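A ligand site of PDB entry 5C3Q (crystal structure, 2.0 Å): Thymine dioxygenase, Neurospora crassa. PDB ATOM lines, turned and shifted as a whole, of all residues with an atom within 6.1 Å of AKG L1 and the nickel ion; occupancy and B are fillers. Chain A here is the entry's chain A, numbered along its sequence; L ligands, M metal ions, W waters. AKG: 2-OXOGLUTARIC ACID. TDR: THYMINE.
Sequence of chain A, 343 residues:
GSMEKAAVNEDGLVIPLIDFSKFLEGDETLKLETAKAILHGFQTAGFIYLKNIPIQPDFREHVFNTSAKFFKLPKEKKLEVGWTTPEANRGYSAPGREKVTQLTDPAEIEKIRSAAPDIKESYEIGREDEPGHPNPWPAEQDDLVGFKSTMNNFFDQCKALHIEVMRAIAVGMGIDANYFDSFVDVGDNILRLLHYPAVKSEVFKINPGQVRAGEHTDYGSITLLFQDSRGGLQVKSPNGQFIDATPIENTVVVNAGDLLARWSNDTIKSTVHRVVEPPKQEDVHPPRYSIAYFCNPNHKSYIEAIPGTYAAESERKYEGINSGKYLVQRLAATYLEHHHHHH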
ATOM      1  N   LYS A 120       2.040  -6.217  -7.846  1.00  0.00           N
ATOM      2  CA  LYS A 120       2.775  -5.533  -8.908  1.00  0.00           C
ATOM      3  C   LYS A 120       3.027  -4.076  -8.548  1.00  0.00           C
ATOM      4  O   LYS A 120       2.364  -3.536  -7.666  1.00  0.00           O
ATOM      5  CB  LYS A 120       1.988  -5.612 -10.223  1.00  0.00           C
ATOM      6  CG  LYS A 120       0.693  -4.787 -10.253  1.00  0.00           C
ATOM      7  CD  LYS A 120       0.025  -4.834 -11.609  1.00  0.00           C
ATOM      8  CE  LYS A 120      -1.200  -3.917 -11.651  1.00  0.00           C
ATOM      9  NZ  LYS A 120      -1.776  -3.836 -13.027  1.00  0.00           N
ATOM     10  N   ARG A 192       4.509   2.080 -19.858  1.00  0.00           N
ATOM     11  CA  ARG A 192       4.298   1.499 -18.529  1.00  0.00           C
ATOM     12  C   ARG A 192       5.385   0.478 -18.198  1.00  0.00           C
ATOM     13  O   ARG A 192       5.426  -0.617 -18.768  1.00  0.00           O
ATOM     14  CB  ARG A 192       2.921   0.841 -18.438  1.00  0.00           C
ATOM     15  CG  ARG A 192       2.620   0.235 -17.075  1.00  0.00           C
ATOM     16  CD  ARG A 192       1.308  -0.529 -17.065  1.00  0.00           C
ATOM     17  NE  ARG A 192       0.222   0.247 -16.492  1.00  0.00           N
ATOM     18  CZ  ARG A 192      -1.011  -0.211 -16.274  1.00  0.00           C
ATOM     19  NH1 ARG A 192      -1.340  -1.461 -16.602  1.00  0.00           N
ATOM     20  NH2 ARG A 192      -1.925   0.590 -15.739  1.00  0.00           N
ATOM     21  N   LEU A 194       6.737  -2.185 -15.637  1.00  0.00           N
ATOM     22  CA  LEU A 194       6.105  -3.078 -14.667  1.00  0.00           C
ATOM     23  C   LEU A 194       7.131  -3.937 -13.943  1.00  0.00           C
ATOM     24  O   LEU A 194       8.047  -4.488 -14.559  1.00  0.00           O
ATOM     25  CB  LEU A 194       5.089  -3.987 -15.355  1.00  0.00           C
ATOM     26  CG  LEU A 194       3.778  -3.313 -15.762  1.00  0.00           C
ATOM     27  CD1 LEU A 194       3.132  -4.040 -16.942  1.00  0.00           C
ATOM     28  CD2 LEU A 194       2.828  -3.259 -14.576  1.00  0.00           C
ATOM     29  N   TYR A 196       6.854  -7.072 -11.079  1.00  0.00           N
ATOM     30  CA  TYR A 196       6.072  -7.980 -10.259  1.00  0.00           C
ATOM     31  C   TYR A 196       7.039  -8.613  -9.260  1.00  0.00           C
ATOM     32  O   TYR A 196       7.832  -9.470  -9.634  1.00  0.00           O
ATOM     33  CB  TYR A 196       5.411  -9.050 -11.122  1.00  0.00           C
ATOM     34  CG  TYR A 196       4.510  -8.522 -12.211  1.00  0.00           C
ATOM     35  CD1 TYR A 196       5.002  -8.199 -13.471  1.00  0.00           C
ATOM     36  CD2 TYR A 196       3.140  -8.343 -11.988  1.00  0.00           C
ATOM     37  CE1 TYR A 196       4.176  -7.705 -14.477  1.00  0.00           C
ATOM     38  CE2 TYR A 196       2.306  -7.862 -12.984  1.00  0.00           C
ATOM     39  CZ  TYR A 196       2.828  -7.542 -14.223  1.00  0.00           C
ATOM     40  OH  TYR A 196       1.986  -7.073 -15.200  1.00  0.00           O
ATOM     41  N   ALA A 213      -1.515  -9.660 -12.345  1.00  0.00           N
ATOM     42  CA  ALA A 213      -2.285  -8.609 -13.016  1.00  0.00           C
ATOM     43  C   ALA A 213      -3.691  -9.121 -13.352  1.00  0.00           C
ATOM     44  O   ALA A 213      -3.833 -10.118 -14.050  1.00  0.00           O
ATOM     45  CB  ALA A 213      -1.593  -8.139 -14.279  1.00  0.00           C
ATOM     46  N   HIS A 216      -8.275  -8.105 -17.970  1.00  0.00           N
ATOM     47  CA  HIS A 216      -8.714  -6.844 -18.532  1.00  0.00           C
ATOM     48  C   HIS A 216      -8.525  -6.835 -20.044  1.00  0.00           C
ATOM     49  O   HIS A 216      -7.892  -7.742 -20.599  1.00  0.00           O
ATOM     50  CB  HIS A 216      -7.896  -5.707 -17.937  1.00  0.00           C
ATOM     51  CG  HIS A 216      -6.450  -5.790 -18.282  1.00  0.00           C
ATOM     52  ND1 HIS A 216      -5.609  -6.727 -17.723  1.00  0.00           N
ATOM     53  CD2 HIS A 216      -5.699  -5.096 -19.172  1.00  0.00           C
ATOM     54  CE1 HIS A 216      -4.395  -6.590 -18.235  1.00  0.00           C
ATOM     55  NE2 HIS A 216      -4.424  -5.616 -19.113  1.00  0.00           N
ATOM     56  N   THR A 217      -9.079  -5.820 -20.692  1.00  0.00           N
ATOM     57  CA  THR A 217      -8.722  -5.470 -22.050  1.00  0.00           C
ATOM     58  C   THR A 217      -7.952  -4.158 -22.014  1.00  0.00           C
ATOM     59  O   THR A 217      -8.177  -3.315 -21.124  1.00  0.00           O
ATOM     60  CB  THR A 217      -9.963  -5.316 -22.954  1.00  0.00           C
ATOM     61  OG1 THR A 217     -10.859  -4.355 -22.392  1.00  0.00           O
ATOM     62  CG2 THR A 217     -10.688  -6.644 -23.118  1.00  0.00           C
ATOM     63  N   ASP A 218      -7.030  -3.975 -22.963  1.00  0.00           N
ATOM     64  CA  ASP A 218      -6.329  -2.708 -23.113  1.00  0.00           C
ATOM     65  C   ASP A 218      -7.239  -1.705 -23.814  1.00  0.00           C
ATOM     66  O   ASP A 218      -8.175  -2.095 -24.508  1.00  0.00           O
ATOM     67  CB  ASP A 218      -5.020  -2.892 -23.901  1.00  0.00           C
ATOM     68  CG  ASP A 218      -3.961  -3.661 -23.112  1.00  0.00           C
ATOM     69  OD1 ASP A 218      -4.150  -3.974 -21.922  1.00  0.00           O
ATOM     70  OD2 ASP A 218      -2.896  -3.955 -23.709  1.00  0.00           O
ATOM     71  N   THR A 223      -0.984  -2.320 -28.071  1.00  0.00           N
ATOM     72  CA  THR A 223      -0.041  -2.340 -26.981  1.00  0.00           C
ATOM     73  C   THR A 223       1.160  -3.149 -27.428  1.00  0.00           C
ATOM     74  O   THR A 223       1.009  -4.223 -28.008  1.00  0.00           O
ATOM     75  CB  THR A 223      -0.642  -2.961 -25.698  1.00  0.00           C
ATOM     76  OG1 THR A 223      -1.777  -2.195 -25.288  1.00  0.00           O
ATOM     77  CG2 THR A 223       0.381  -2.981 -24.562  1.00  0.00           C
ATOM     78  N   LEU A 225       3.998  -5.157 -25.883  1.00  0.00           N
ATOM     79  CA  LEU A 225       4.349  -5.773 -24.611  1.00  0.00           C
ATOM     80  C   LEU A 225       5.673  -6.515 -24.707  1.00  0.00           C
ATOM     81  O   LEU A 225       5.782  -7.517 -25.419  1.00  0.00           O
ATOM     82  CB  LEU A 225       3.252  -6.727 -24.143  1.00  0.00           C
ATOM     83  CG  LEU A 225       3.553  -7.338 -22.763  1.00  0.00           C
ATOM     84  CD1 LEU A 225       3.312  -6.338 -21.648  1.00  0.00           C
ATOM     85  CD2 LEU A 225       2.728  -8.587 -22.540  1.00  0.00           C
ATOM     86  N   PHE A 226       6.669  -6.006 -23.994  1.00  0.00           N
ATOM     87  CA  PHE A 226       7.969  -6.634 -23.897  1.00  0.00           C
ATOM     88  C   PHE A 226       8.008  -7.376 -22.559  1.00  0.00           C
ATOM     89  O   PHE A 226       7.863  -6.764 -21.502  1.00  0.00           O
ATOM     90  CB  PHE A 226       9.068  -5.564 -23.930  1.00  0.00           C
ATOM     91  CG  PHE A 226       9.019  -4.662 -25.143  1.00  0.00           C
ATOM     92  CD1 PHE A 226       8.202  -3.534 -25.151  1.00  0.00           C
ATOM     93  CD2 PHE A 226       9.783  -4.932 -26.258  1.00  0.00           C
ATOM     94  CE1 PHE A 226       8.152  -2.697 -26.246  1.00  0.00           C
ATOM     95  CE2 PHE A 226       9.736  -4.104 -27.373  1.00  0.00           C
ATOM     96  CZ  PHE A 226       8.921  -2.986 -27.362  1.00  0.00           C
ATOM     97  N   GLN A 227       8.156  -8.702 -22.609  1.00  0.00           N
ATOM     98  CA  GLN A 227       8.207  -9.501 -21.382  1.00  0.00           C
ATOM     99  C   GLN A 227       9.541 -10.224 -21.266  1.00  0.00           C
ATOM    100  O   GLN A 227      10.168 -10.553 -22.282  1.00  0.00           O
ATOM    101  CB  GLN A 227       7.032 -10.488 -21.311  1.00  0.00           C
ATOM    102  CG  GLN A 227       7.004 -11.581 -22.376  1.00  0.00           C
ATOM    103  CD  GLN A 227       5.840 -12.558 -22.194  1.00  0.00           C
ATOM    104  OE1 GLN A 227       5.317 -12.720 -21.099  1.00  0.00           O
ATOM    105  NE2 GLN A 227       5.450 -13.219 -23.275  1.00  0.00           N
ATOM    106  N   LEU A 233       1.855 -14.485 -18.361  1.00  0.00           N
ATOM    107  CA  LEU A 233       0.882 -13.826 -19.229  1.00  0.00           C
ATOM    108  C   LEU A 233      -0.034 -14.854 -19.876  1.00  0.00           C
ATOM    109  O   LEU A 233       0.428 -15.869 -20.396  1.00  0.00           O
ATOM    110  CB  LEU A 233       1.579 -12.997 -20.308  1.00  0.00           C
ATOM    111  CG  LEU A 233       0.671 -12.338 -21.353  1.00  0.00           C
ATOM    112  CD1 LEU A 233      -0.217 -11.273 -20.717  1.00  0.00           C
ATOM    113  CD2 LEU A 233       1.503 -11.731 -22.472  1.00  0.00           C
ATOM    114  N   ASN A 255      -0.864  -6.532 -29.072  1.00  0.00           N
ATOM    115  CA  ASN A 255      -2.298  -6.760 -29.049  1.00  0.00           C
ATOM    116  C   ASN A 255      -3.081  -5.492 -29.332  1.00  0.00           C
ATOM    117  O   ASN A 255      -2.673  -4.398 -28.945  1.00  0.00           O
ATOM    118  CB  ASN A 255      -2.721  -7.366 -27.715  1.00  0.00           C
ATOM    119  CG  ASN A 255      -2.528  -6.417 -26.544  1.00  0.00           C
ATOM    120  OD1 ASN A 255      -1.407  -6.232 -26.077  1.00  0.00           O
ATOM    121  ND2 ASN A 255      -3.611  -5.826 -26.058  1.00  0.00           N
ATOM    122  N   HIS A 273      -6.836 -10.521 -21.289  1.00  0.00           N
ATOM    123  CA  HIS A 273      -5.599 -11.121 -20.844  1.00  0.00           C
ATOM    124  C   HIS A 273      -5.309 -10.774 -19.389  1.00  0.00           C
ATOM    125  O   HIS A 273      -5.920  -9.872 -18.822  1.00  0.00           O
ATOM    126  CB  HIS A 273      -4.433 -10.699 -21.748  1.00  0.00           C
ATOM    127  CG  HIS A 273      -4.325  -9.217 -21.937  1.00  0.00           C
ATOM    128  ND1 HIS A 273      -5.255  -8.487 -22.650  1.00  0.00           N
ATOM    129  CD2 HIS A 273      -3.397  -8.337 -21.496  1.00  0.00           C
ATOM    130  CE1 HIS A 273      -4.899  -7.213 -22.640  1.00  0.00           C
ATOM    131  NE2 HIS A 273      -3.787  -7.096 -21.945  1.00  0.00           N
ATOM    132  N   ARG A 274      -4.378 -11.511 -18.787  1.00  0.00           N
ATOM    133  CA  ARG A 274      -4.053 -11.360 -17.378  1.00  0.00           C
ATOM    134  C   ARG A 274      -2.637 -11.878 -17.139  1.00  0.00           C
ATOM    135  O   ARG A 274      -2.018 -12.440 -18.044  1.00  0.00           O
ATOM    136  CB  ARG A 274      -5.047 -12.150 -16.506  1.00  0.00           C
ATOM    137  CG  ARG A 274      -4.890 -13.659 -16.593  1.00  0.00           C
ATOM    138  CD  ARG A 274      -6.031 -14.392 -15.899  1.00  0.00           C
ATOM    139  NE  ARG A 274      -5.814 -15.835 -15.909  1.00  0.00           N
ATOM    140  CZ  ARG A 274      -6.550 -16.718 -15.245  1.00  0.00           C
ATOM    141  NH1 ARG A 274      -7.579 -16.324 -14.502  1.00  0.00           N
ATOM    142  NH2 ARG A 274      -6.254 -18.014 -15.315  1.00  0.00           N
ATOM    143  N   VAL A 275      -2.134 -11.676 -15.927  1.00  0.00           N
ATOM    144  CA  VAL A 275      -0.874 -12.280 -15.511  1.00  0.00           C
ATOM    145  C   VAL A 275      -1.098 -13.039 -14.209  1.00  0.00           C
ATOM    146  O   VAL A 275      -1.570 -12.461 -13.225  1.00  0.00           O
ATOM    147  CB  VAL A 275       0.250 -11.250 -15.323  1.00  0.00           C
ATOM    148  CG1 VAL A 275       1.577 -11.947 -15.046  1.00  0.00           C
ATOM    149  CG2 VAL A 275       0.396 -10.367 -16.564  1.00  0.00           C
ATOM    150  N   ARG A 288       9.371 -10.661 -11.788  1.00  0.00           N
ATOM    151  CA  ARG A 288       9.057 -10.581 -13.208  1.00  0.00           C
ATOM    152  C   ARG A 288       9.030  -9.109 -13.647  1.00  0.00           C
ATOM    153  O   ARG A 288       8.426  -8.259 -12.991  1.00  0.00           O
ATOM    154  CB  ARG A 288       7.709 -11.245 -13.507  1.00  0.00           C
ATOM    155  CG  ARG A 288       7.203 -11.060 -14.935  1.00  0.00           C
ATOM    156  CD  ARG A 288       6.037 -11.975 -15.252  1.00  0.00           C
ATOM    157  NE  ARG A 288       5.689 -11.956 -16.677  1.00  0.00           N
ATOM    158  CZ  ARG A 288       4.928 -11.039 -17.271  1.00  0.00           C
ATOM    159  NH1 ARG A 288       4.412 -10.021 -16.583  1.00  0.00           N
ATOM    160  NH2 ARG A 288       4.685 -11.139 -18.573  1.00  0.00           N
ATOM    161  N   SER A 290       8.165  -6.590 -16.965  1.00  0.00           N
ATOM    162  CA  SER A 290       7.653  -6.368 -18.302  1.00  0.00           C
ATOM    163  C   SER A 290       7.514  -4.879 -18.546  1.00  0.00           C
ATOM    164  O   SER A 290       7.583  -4.062 -17.609  1.00  0.00           O
ATOM    165  CB  SER A 290       6.299  -7.077 -18.493  1.00  0.00           C
ATOM    166  OG  SER A 290       5.306  -6.531 -17.652  1.00  0.00           O
ATOM    167  N   ILE A 291       7.358  -4.532 -19.816  1.00  0.00           N
ATOM    168  CA  ILE A 291       7.139  -3.163 -20.230  1.00  0.00           C
ATOM    169  C   ILE A 291       5.965  -3.167 -21.196  1.00  0.00           C
ATOM    170  O   ILE A 291       6.016  -3.814 -22.259  1.00  0.00           O
ATOM    171  CB  ILE A 291       8.385  -2.559 -20.903  1.00  0.00           C
ATOM    172  CG1 ILE A 291       9.587  -2.651 -19.959  1.00  0.00           C
ATOM    173  CG2 ILE A 291       8.114  -1.111 -21.307  1.00  0.00           C
ATOM    174  CD1 ILE A 291      10.900  -2.165 -20.552  1.00  0.00           C
ATOM    175  N   ALA A 292       4.892  -2.467 -20.825  1.00  0.00           N
ATOM    176  CA  ALA A 292       3.743  -2.278 -21.701  1.00  0.00           C
ATOM    177  C   ALA A 292       3.774  -0.871 -22.269  1.00  0.00           C
ATOM    178  O   ALA A 292       3.668   0.110 -21.527  1.00  0.00           O
ATOM    179  CB  ALA A 292       2.454  -2.513 -20.937  1.00  0.00           C
ATOM    180  N   PHE A 294       1.573   1.387 -24.216  1.00  0.00           N
ATOM    181  CA  PHE A 294       0.204   1.591 -24.674  1.00  0.00           C
ATOM    182  C   PHE A 294       0.195   2.626 -25.779  1.00  0.00           C
ATOM    183  O   PHE A 294       0.545   3.791 -25.554  1.00  0.00           O
ATOM    184  CB  PHE A 294      -0.688   2.064 -23.529  1.00  0.00           C
ATOM    185  CG  PHE A 294      -0.767   1.109 -22.376  1.00  0.00           C
ATOM    186  CD1 PHE A 294      -1.253  -0.176 -22.564  1.00  0.00           C
ATOM    187  CD2 PHE A 294      -0.380   1.496 -21.104  1.00  0.00           C
ATOM    188  CE1 PHE A 294      -1.343  -1.061 -21.500  1.00  0.00           C
ATOM    189  CE2 PHE A 294      -0.461   0.614 -20.039  1.00  0.00           C
ATOM    190  CZ  PHE A 294      -0.946  -0.671 -20.237  1.00  0.00           C
HETATM  191  C1  AKG L   1      -0.908  -4.364 -18.838  1.00  0.00           C
HETATM  192  O1  AKG L   1      -1.948  -3.895 -19.377  1.00  0.00           O
HETATM  193  O2  AKG L   1      -0.157  -3.671 -18.124  1.00  0.00           O
HETATM  194  C2  AKG L   1      -0.579  -5.783 -19.051  1.00  0.00           C
HETATM  195  O5  AKG L   1      -1.379  -6.523 -19.609  1.00  0.00           O
HETATM  196  C3  AKG L   1       0.762  -6.316 -18.567  1.00  0.00           C
HETATM  197  C4  AKG L   1       0.971  -7.762 -19.029  1.00  0.00           C
HETATM  198  C5  AKG L   1       2.333  -8.276 -18.623  1.00  0.00           C
HETATM  199  O3  AKG L   1       2.826  -9.207 -19.308  1.00  0.00           O
HETATM  200  O4  AKG L   1       2.930  -7.786 -17.635  1.00  0.00           O
HETATM  201  N1  TDR L   2      -3.444   2.226 -18.821  1.00  0.00           N
HETATM  202  C2  TDR L   2      -3.474   2.815 -20.144  1.00  0.00           C
HETATM  203  O2  TDR L   2      -3.113   3.960 -20.300  1.00  0.00           O
HETATM  204  N3  TDR L   2      -3.930   2.023 -21.265  1.00  0.00           N
HETATM  205  C4  TDR L   2      -4.353   0.675 -21.090  1.00  0.00           C
HETATM  206  O4  TDR L   2      -4.729   0.046 -22.059  1.00  0.00           O
HETATM  207  C5  TDR L   2      -4.331   0.073 -19.748  1.00  0.00           C
HETATM  208  CM5 TDR L   2      -4.775  -1.334 -19.497  1.00  0.00           C
HETATM  209  C6  TDR L   2      -3.869   0.877 -18.616  1.00  0.00           C
HETATM  210 NI    NI M   1      -2.943  -5.405 -20.738  1.00  0.00          NI
HETATM  211  O   HOH W   1      -3.580  -3.430 -16.844  1.00  0.00           O
HETATM  212  O   HOH W   2      -0.185  -4.864 -15.353  1.00  0.00           O
HETATM  213  O   HOH W   3      -1.293  -5.174 -22.191  1.00  0.00           O
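Three residues have an atom within 4 Å of the nickel ion: His 216, Asp 218 and His 273.
The nearest printed residue that does not touch the nickel ion is Phe 294 (4.7 Å).
OG of Ser 290 sits at hydrogen-bond distance from O4 of AKG L1 (2.7 Å).
An oxygen (O4) of AKG L1 sits at hydrogen-bond distance from the side-chain hydroxyl (OH) of Tyr 196.
The guanidinium group (NH2) of Arg 288 lies within salt-bridge range of an oxygen (O3) of AKG L1, 2.8 Å away.
An oxygen (O2) of AKG L1 lies within salt-bridge range of the guanidinium group (NH1) of Arg 192, at 2.9 Å.
Merely in contact with AKG L1: Leu 194, Leu 225, Leu 233, Val 275 and Phe 294.
The nearest printed residue that does not touch AKG L1 is Ala 292 (4.01 Å).
The side-chain carboxylate (OD2) of Asp 218 lies within hydrogen-bond range of the side-chain amide nitrogen (ND2) of Asn 255, 3.1 Å away.
OD2 of Asp 218 lies within hydrogen-bond range of OG1 of Thr 223, 2.6 Å away.
O of Ser 290 is in hydrogen-bond range of N of Leu 194 (2.9 Å).
O of Arg 288 sits at hydrogen-bond distance from N of Tyr 196 (2.7 Å).
NH2 of Arg 288 lies within hydrogen-bond range of OE1 of Gln 227, 3.0 Å away.
N of Arg 192 is in hydrogen-bond range of O of Ala 292, 2.7 Å away.
The backbone carbonyl oxygen (O) of Val 275 sits at hydrogen-bond distance from the backbone NH (N) of Ala 213 (2.9 Å).
Water W2 lies within hydrogen-bond range of the side-chain amino group of Lys 120 (3.0 Å), an oxygen (O2) of AKG L1 (3.0 Å) and the side-chain hydroxyl of Tyr 196 (3.1 Å).
The nickel ion is bound by NE2 of His 216 (2.2 Å), water W3 (2.2 Å), OD1 of Asp 218 (2.2 Å), O5 of AKG L1 (2.2 Å), NE2 of His 273 (2.2 Å) and O1 of AKG L1 (2.3 Å).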
